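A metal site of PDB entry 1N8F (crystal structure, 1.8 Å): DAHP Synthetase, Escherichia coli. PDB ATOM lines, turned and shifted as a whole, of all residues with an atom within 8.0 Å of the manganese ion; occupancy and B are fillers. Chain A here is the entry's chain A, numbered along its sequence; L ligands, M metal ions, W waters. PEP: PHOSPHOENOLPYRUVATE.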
ATOM      1  N   GLY A  59      15.678 -10.417   0.575  1.00  0.00           N
ATOM      2  CA  GLY A  59      16.458 -10.063   1.749  1.00  0.00           C
ATOM      3  C   GLY A  59      17.106  -8.696   1.634  1.00  0.00           C
ATOM      4  O   GLY A  59      16.846  -7.964   0.675  1.00  0.00           O
ATOM      5  N   PRO A  60      17.963  -8.332   2.590  1.00  0.00           N
ATOM      6  CA  PRO A  60      18.643  -7.032   2.579  1.00  0.00           C
ATOM      7  C   PRO A  60      19.439  -6.785   1.295  1.00  0.00           C
ATOM      8  O   PRO A  60      19.851  -7.725   0.613  1.00  0.00           O
ATOM      9  CB  PRO A  60      19.567  -7.116   3.793  1.00  0.00           C
ATOM     10  CG  PRO A  60      18.799  -8.015   4.726  1.00  0.00           C
ATOM     11  CD  PRO A  60      18.316  -9.096   3.800  1.00  0.00           C
ATOM     12  N   CYS A  61      19.634  -5.511   0.974  1.00  0.00           N
ATOM     13  CA  CYS A  61      20.414  -5.145  -0.195  1.00  0.00           C
ATOM     14  C   CYS A  61      21.832  -5.617   0.113  1.00  0.00           C
ATOM     15  O   CYS A  61      22.537  -6.129  -0.757  1.00  0.00           O
ATOM     16  CB  CYS A  61      20.416  -3.628  -0.394  1.00  0.00           C
ATOM     17  SG  CYS A  61      21.642  -3.066  -1.607  1.00  0.00           S
ATOM     18  N   SER A  62      22.218  -5.445   1.372  1.00  0.00           N
ATOM     19  CA  SER A  62      23.545  -5.852   1.842  1.00  0.00           C
ATOM     20  C   SER A  62      23.515  -6.198   3.316  1.00  0.00           C
ATOM     21  O   SER A  62      22.696  -5.663   4.070  1.00  0.00           O
ATOM     22  CB  SER A  62      24.560  -4.729   1.625  1.00  0.00           C
ATOM     23  OG  SER A  62      24.253  -3.598   2.427  1.00  0.00           O
ATOM     24  N   ARG A  92      18.591 -13.259   0.617  1.00  0.00           N
ATOM     25  CA  ARG A  92      19.669 -12.490   0.011  1.00  0.00           C
ATOM     26  C   ARG A  92      20.674 -12.280   1.136  1.00  0.00           C
ATOM     27  O   ARG A  92      20.382 -11.587   2.111  1.00  0.00           O
ATOM     28  CB  ARG A  92      19.173 -11.112  -0.462  1.00  0.00           C
ATOM     29  CG  ARG A  92      18.491 -11.077  -1.814  1.00  0.00           C
ATOM     30  CD  ARG A  92      18.094  -9.645  -2.167  1.00  0.00           C
ATOM     31  NE  ARG A  92      19.232  -8.732  -2.095  1.00  0.00           N
ATOM     32  CZ  ARG A  92      19.778  -8.128  -3.137  1.00  0.00           C
ATOM     33  NH1 ARG A  92      19.312  -8.323  -4.363  1.00  0.00           N
ATOM     34  NH2 ARG A  92      20.817  -7.327  -2.956  1.00  0.00           N
ATOM     35  N   TYR A  94      23.979 -10.940   0.828  1.00  0.00           N
ATOM     36  CA  TYR A  94      24.997 -10.244   0.037  1.00  0.00           C
ATOM     37  C   TYR A  94      26.145  -9.630   0.815  1.00  0.00           C
ATOM     38  O   TYR A  94      25.966  -8.638   1.529  1.00  0.00           O
ATOM     39  CB  TYR A  94      24.325  -9.178  -0.820  1.00  0.00           C
ATOM     40  CG  TYR A  94      23.584  -9.726  -2.033  1.00  0.00           C
ATOM     41  CD1 TYR A  94      22.697 -10.793  -1.903  1.00  0.00           C
ATOM     42  CD2 TYR A  94      23.768  -9.156  -3.296  1.00  0.00           C
ATOM     43  CE1 TYR A  94      22.010 -11.287  -3.022  1.00  0.00           C
ATOM     44  CE2 TYR A  94      23.088  -9.644  -4.404  1.00  0.00           C
ATOM     45  CZ  TYR A  94      22.209 -10.705  -4.265  1.00  0.00           C
ATOM     46  OH  TYR A  94      21.537 -11.186  -5.362  1.00  0.00           O
ATOM     47  N   LYS A  97      29.374  -5.733  -2.641  1.00  0.00           N
ATOM     48  CA  LYS A  97      28.600  -4.717  -3.355  1.00  0.00           C
ATOM     49  C   LYS A  97      29.375  -3.934  -4.410  1.00  0.00           C
ATOM     50  O   LYS A  97      30.426  -3.348  -4.128  1.00  0.00           O
ATOM     51  CB  LYS A  97      28.023  -3.722  -2.333  1.00  0.00           C
ATOM     52  CG  LYS A  97      27.226  -4.367  -1.200  1.00  0.00           C
ATOM     53  CD  LYS A  97      26.085  -5.210  -1.730  1.00  0.00           C
ATOM     54  CE  LYS A  97      25.050  -4.362  -2.454  1.00  0.00           C
ATOM     55  NZ  LYS A  97      23.955  -5.198  -3.011  1.00  0.00           N
ATOM     56  N   PRO A  98      28.855  -3.905  -5.652  1.00  0.00           N
ATOM     57  CA  PRO A  98      29.504  -3.183  -6.752  1.00  0.00           C
ATOM     58  C   PRO A  98      29.033  -1.729  -6.676  1.00  0.00           C
ATOM     59  O   PRO A  98      27.838  -1.473  -6.550  1.00  0.00           O
ATOM     60  CB  PRO A  98      28.964  -3.891  -7.986  1.00  0.00           C
ATOM     61  CG  PRO A  98      27.558  -4.200  -7.582  1.00  0.00           C
ATOM     62  CD  PRO A  98      27.720  -4.706  -6.152  1.00  0.00           C
ATOM     63  N   GLU A 143      25.742 -12.096  -4.532  1.00  0.00           N
ATOM     64  CA  GLU A 143      26.362 -11.731  -5.797  1.00  0.00           C
ATOM     65  C   GLU A 143      27.807 -12.182  -5.775  1.00  0.00           C
ATOM     66  O   GLU A 143      28.530 -11.960  -4.803  1.00  0.00           O
ATOM     67  CB  GLU A 143      26.346 -10.222  -6.047  1.00  0.00           C
ATOM     68  CG  GLU A 143      26.993  -9.860  -7.408  1.00  0.00           C
ATOM     69  CD  GLU A 143      27.120  -8.369  -7.674  1.00  0.00           C
ATOM     70  OE1 GLU A 143      26.272  -7.596  -7.168  1.00  0.00           O
ATOM     71  OE2 GLU A 143      28.055  -7.979  -8.414  1.00  0.00           O
ATOM     72  N   ARG A 165      26.592  -4.732 -13.755  1.00  0.00           N
ATOM     73  CA  ARG A 165      27.858  -4.121 -14.160  1.00  0.00           C
ATOM     74  C   ARG A 165      28.945  -5.123 -14.519  1.00  0.00           C
ATOM     75  O   ARG A 165      30.021  -4.728 -14.987  1.00  0.00           O
ATOM     76  CB  ARG A 165      28.356  -3.203 -13.041  1.00  0.00           C
ATOM     77  CG  ARG A 165      27.335  -2.143 -12.677  1.00  0.00           C
ATOM     78  CD  ARG A 165      27.755  -1.331 -11.457  1.00  0.00           C
ATOM     79  NE  ARG A 165      26.696  -0.396 -11.098  1.00  0.00           N
ATOM     80  CZ  ARG A 165      25.538  -0.741 -10.542  1.00  0.00           C
ATOM     81  NH1 ARG A 165      25.273  -2.018 -10.284  1.00  0.00           N
ATOM     82  NH2 ARG A 165      24.629   0.185 -10.276  1.00  0.00           N
ATOM     83  N   LYS A 186      22.147 -10.577 -14.488  1.00  0.00           N
ATOM     84  CA  LYS A 186      21.347  -9.371 -14.616  1.00  0.00           C
ATOM     85  C   LYS A 186      21.582  -8.688 -15.956  1.00  0.00           C
ATOM     86  O   LYS A 186      22.678  -8.750 -16.505  1.00  0.00           O
ATOM     87  CB  LYS A 186      21.671  -8.414 -13.481  1.00  0.00           C
ATOM     88  CG  LYS A 186      21.227  -8.943 -12.130  1.00  0.00           C
ATOM     89  CD  LYS A 186      21.181  -7.845 -11.120  1.00  0.00           C
ATOM     90  CE  LYS A 186      20.138  -8.130 -10.061  1.00  0.00           C
ATOM     91  NZ  LYS A 186      19.915  -6.909  -9.249  1.00  0.00           N
ATOM     92  N   ARG A 234      16.242  -6.472 -14.288  1.00  0.00           N
ATOM     93  CA  ARG A 234      16.359  -5.496 -13.207  1.00  0.00           C
ATOM     94  C   ARG A 234      16.191  -4.060 -13.692  1.00  0.00           C
ATOM     95  O   ARG A 234      16.585  -3.111 -13.011  1.00  0.00           O
ATOM     96  CB  ARG A 234      17.707  -5.662 -12.487  1.00  0.00           C
ATOM     97  CG  ARG A 234      18.937  -5.723 -13.398  1.00  0.00           C
ATOM     98  CD  ARG A 234      19.394  -4.341 -13.848  1.00  0.00           C
ATOM     99  NE  ARG A 234      20.044  -3.603 -12.762  1.00  0.00           N
ATOM    100  CZ  ARG A 234      20.280  -2.299 -12.781  1.00  0.00           C
ATOM    101  NH1 ARG A 234      19.912  -1.572 -13.823  1.00  0.00           N
ATOM    102  NH2 ARG A 234      20.904  -1.717 -11.767  1.00  0.00           N
ATOM    103  N   ASP A 265      13.627  -8.862 -10.996  1.00  0.00           N
ATOM    104  CA  ASP A 265      14.069  -8.149  -9.801  1.00  0.00           C
ATOM    105  C   ASP A 265      13.081  -6.996  -9.643  1.00  0.00           C
ATOM    106  O   ASP A 265      12.904  -6.200 -10.564  1.00  0.00           O
ATOM    107  CB  ASP A 265      15.489  -7.608 -10.024  1.00  0.00           C
ATOM    108  CG  ASP A 265      16.027  -6.799  -8.849  1.00  0.00           C
ATOM    109  OD1 ASP A 265      15.308  -6.625  -7.844  1.00  0.00           O
ATOM    110  OD2 ASP A 265      17.182  -6.332  -8.941  1.00  0.00           O
ATOM    111  N   SER A 267      13.352  -4.626  -7.447  1.00  0.00           N
ATOM    112  CA  SER A 267      14.078  -3.453  -6.997  1.00  0.00           C
ATOM    113  C   SER A 267      14.973  -2.791  -8.048  1.00  0.00           C
ATOM    114  O   SER A 267      14.812  -3.005  -9.251  1.00  0.00           O
ATOM    115  CB  SER A 267      14.890  -3.802  -5.748  1.00  0.00           C
ATOM    116  OG  SER A 267      15.210  -2.631  -5.000  1.00  0.00           O
ATOM    117  N   HIS A 268      15.915  -1.993  -7.560  1.00  0.00           N
ATOM    118  CA  HIS A 268      16.861  -1.265  -8.395  1.00  0.00           C
ATOM    119  C   HIS A 268      16.179  -0.457  -9.489  1.00  0.00           C
ATOM    120  O   HIS A 268      15.339   0.391  -9.179  1.00  0.00           O
ATOM    121  CB  HIS A 268      17.902  -2.233  -8.964  1.00  0.00           C
ATOM    122  CG  HIS A 268      18.588  -3.041  -7.911  1.00  0.00           C
ATOM    123  ND1 HIS A 268      18.167  -4.296  -7.543  1.00  0.00           N
ATOM    124  CD2 HIS A 268      19.603  -2.724  -7.063  1.00  0.00           C
ATOM    125  CE1 HIS A 268      18.880  -4.723  -6.515  1.00  0.00           C
ATOM    126  NE2 HIS A 268      19.759  -3.779  -6.214  1.00  0.00           N
ATOM    127  N   MET A 300      13.150 -11.283  -7.360  1.00  0.00           N
ATOM    128  CA  MET A 300      14.137 -10.813  -6.417  1.00  0.00           C
ATOM    129  C   MET A 300      13.552  -9.597  -5.736  1.00  0.00           C
ATOM    130  O   MET A 300      12.987  -8.739  -6.391  1.00  0.00           O
ATOM    131  CB  MET A 300      15.424 -10.434  -7.146  1.00  0.00           C
ATOM    132  CG  MET A 300      16.498  -9.843  -6.271  1.00  0.00           C
ATOM    133  SD  MET A 300      17.990  -9.518  -7.233  1.00  0.00           S
ATOM    134  CE  MET A 300      18.714 -11.151  -7.252  1.00  0.00           C
ATOM    135  N   GLU A 302      14.243  -6.630  -2.405  1.00  0.00           N
ATOM    136  CA  GLU A 302      15.109  -6.088  -1.378  1.00  0.00           C
ATOM    137  C   GLU A 302      14.235  -5.772  -0.190  1.00  0.00           C
ATOM    138  O   GLU A 302      13.398  -4.862  -0.221  1.00  0.00           O
ATOM    139  CB  GLU A 302      15.838  -4.841  -1.888  1.00  0.00           C
ATOM    140  CG  GLU A 302      16.862  -5.198  -2.967  1.00  0.00           C
ATOM    141  CD  GLU A 302      17.858  -4.094  -3.256  1.00  0.00           C
ATOM    142  OE1 GLU A 302      17.441  -2.997  -3.667  1.00  0.00           O
ATOM    143  OE2 GLU A 302      19.066  -4.332  -3.082  1.00  0.00           O
ATOM    144  N   SER A 323      18.808  -0.955   6.230  1.00  0.00           N
ATOM    145  CA  SER A 323      19.853  -0.993   5.198  1.00  0.00           C
ATOM    146  C   SER A 323      20.766   0.230   5.141  1.00  0.00           C
ATOM    147  O   SER A 323      20.307   1.370   5.289  1.00  0.00           O
ATOM    148  CB  SER A 323      19.201  -1.184   3.824  1.00  0.00           C
ATOM    149  OG  SER A 323      20.170  -1.191   2.790  1.00  0.00           O
ATOM    150  N   THR A 325      22.706   0.501   2.454  1.00  0.00           N
ATOM    151  CA  THR A 325      22.889   0.645   1.008  1.00  0.00           C
ATOM    152  C   THR A 325      21.532   0.977   0.380  1.00  0.00           C
ATOM    153  O   THR A 325      20.955   2.014   0.726  1.00  0.00           O
ATOM    154  CB  THR A 325      23.505  -0.626   0.366  1.00  0.00           C
ATOM    155  OG1 THR A 325      22.844  -1.806   0.845  1.00  0.00           O
ATOM    156  CG2 THR A 325      24.993  -0.716   0.715  1.00  0.00           C
ATOM    157  N   ASP A 326      21.007   0.132  -0.500  1.00  0.00           N
ATOM    158  CA  ASP A 326      19.711   0.439  -1.119  1.00  0.00           C
ATOM    159  C   ASP A 326      18.550   0.309  -0.145  1.00  0.00           C
ATOM    160  O   ASP A 326      18.575  -0.541   0.755  1.00  0.00           O
ATOM    161  CB  ASP A 326      19.422  -0.452  -2.330  1.00  0.00           C
ATOM    162  CG  ASP A 326      20.356  -0.183  -3.493  1.00  0.00           C
ATOM    163  OD1 ASP A 326      20.826   0.970  -3.632  1.00  0.00           O
ATOM    164  OD2 ASP A 326      20.593  -1.118  -4.283  1.00  0.00           O
ATOM    165  N   ALA A 327      17.534   1.138  -0.337  1.00  0.00           N
ATOM    166  CA  ALA A 327      16.348   1.123   0.509  1.00  0.00           C
ATOM    167  C   ALA A 327      15.577  -0.169   0.270  1.00  0.00           C
ATOM    168  O   ALA A 327      15.464  -0.634  -0.867  1.00  0.00           O
ATOM    169  CB  ALA A 327      15.479   2.340   0.211  1.00  0.00           C
ATOM    170  N   CYS A 328      15.039  -0.739   1.354  1.00  0.00           N
ATOM    171  CA  CYS A 328      14.280  -1.977   1.288  1.00  0.00           C
ATOM    172  C   CYS A 328      12.873  -1.784   1.860  1.00  0.00           C
ATOM    173  O   CYS A 328      12.605  -0.790   2.540  1.00  0.00           O
ATOM    174  CB  CYS A 328      14.959  -3.077   2.103  1.00  0.00           C
ATOM    175  SG  CYS A 328      16.654  -3.518   1.635  1.00  0.00           S
HETATM  176  C1  PEP L   1      21.909  -6.201  -6.197  1.00  0.00           C
HETATM  177  O1  PEP L   1      22.101  -5.806  -4.989  1.00  0.00           O
HETATM  178  O2' PEP L   1      21.148  -7.092  -6.480  1.00  0.00           O
HETATM  179  C2  PEP L   1      22.708  -5.434  -7.240  1.00  0.00           C
HETATM  180  C3  PEP L   1      23.979  -4.952  -7.163  1.00  0.00           C
HETATM  181  O2  PEP L   1      21.966  -5.196  -8.407  1.00  0.00           O
HETATM  182  P   PEP L   1      22.439  -4.685  -9.846  1.00  0.00           P
HETATM  183  O1P PEP L   1      23.637  -5.572 -10.258  1.00  0.00           O
HETATM  184  O2P PEP L   1      22.768  -3.238  -9.639  1.00  0.00           O
HETATM  185  O3P PEP L   1      21.318  -4.962 -10.777  1.00  0.00           O
HETATM  186 MN    MN M   1      20.620  -3.235  -4.008  1.00  0.00          MN
HETATM  187  O   HOH W   1      22.908  -3.128  -4.605  1.00  0.00           O
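Lys 97 touches the manganese ion. Five residues have an atom within 4 Å of the manganese ion: Cys 61, Lys 97, His 268, Glu 302 and Asp 326.
Water W1 bridges NZ of Lys 97 (2.8 Å) and O1 of the ligand (2.8 Å).
NE2 of His 268 sits close to O1 of the ligand. NZ of Lys 97 is in salt-bridge range of O1 of the ligand. O1 of the ligand is in salt-bridge range of NH2 of Arg 92. The side-chain amino group of Lys 186 is in salt-bridge range of an oxygen (O3P) of the ligand. The guanidinium group (NH1) of Arg 165 lies within salt-bridge range of an oxygen (O2P) of the ligand (2.9 Å). The guanidinium group (NE) of Arg 234 lies within salt-bridge range of an oxygen (O3P) of the ligand, at 2.7 Å.
NH2 of Arg 92 sits close to OE2 of Glu 302, 3.5 Å away. OE1 of Glu 302 sits at hydrogen-bond distance from OG of Ser 267 (2.6 Å). O of Asp 326 sits at hydrogen-bond distance from SG of Cys 328 (3.7 Å). The backbone carbonyl oxygen of Asp 326 is in hydrogen-bond range of the side-chain hydroxyl of Ser 323, 2.7 Å away. The backbone carbonyl oxygen (O) of Cys 61 is in hydrogen-bond range of the side-chain amino group (NZ) of Lys 97. The guanidinium group (NH2) of Arg 92 sits at hydrogen-bond distance from the backbone carbonyl oxygen (O) of Cys 61, 3.0 Å away. The side-chain sulfur (SG) of Cys 61 lies close to the side-chain hydroxyl (OG1) of Thr 325, at 3.0 Å. N of Cys 61 is in hydrogen-bond range of SG of Cys 328, at 3.6 Å.
The manganese ion is bound by the side-chain carboxylate of Glu 302, the side-chain carboxylate of Asp 326, water W1, a ring nitrogen (NE2) of His 268 and the side-chain sulfur of Cys 61. The manganese ion has five donor atoms within binding distance.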
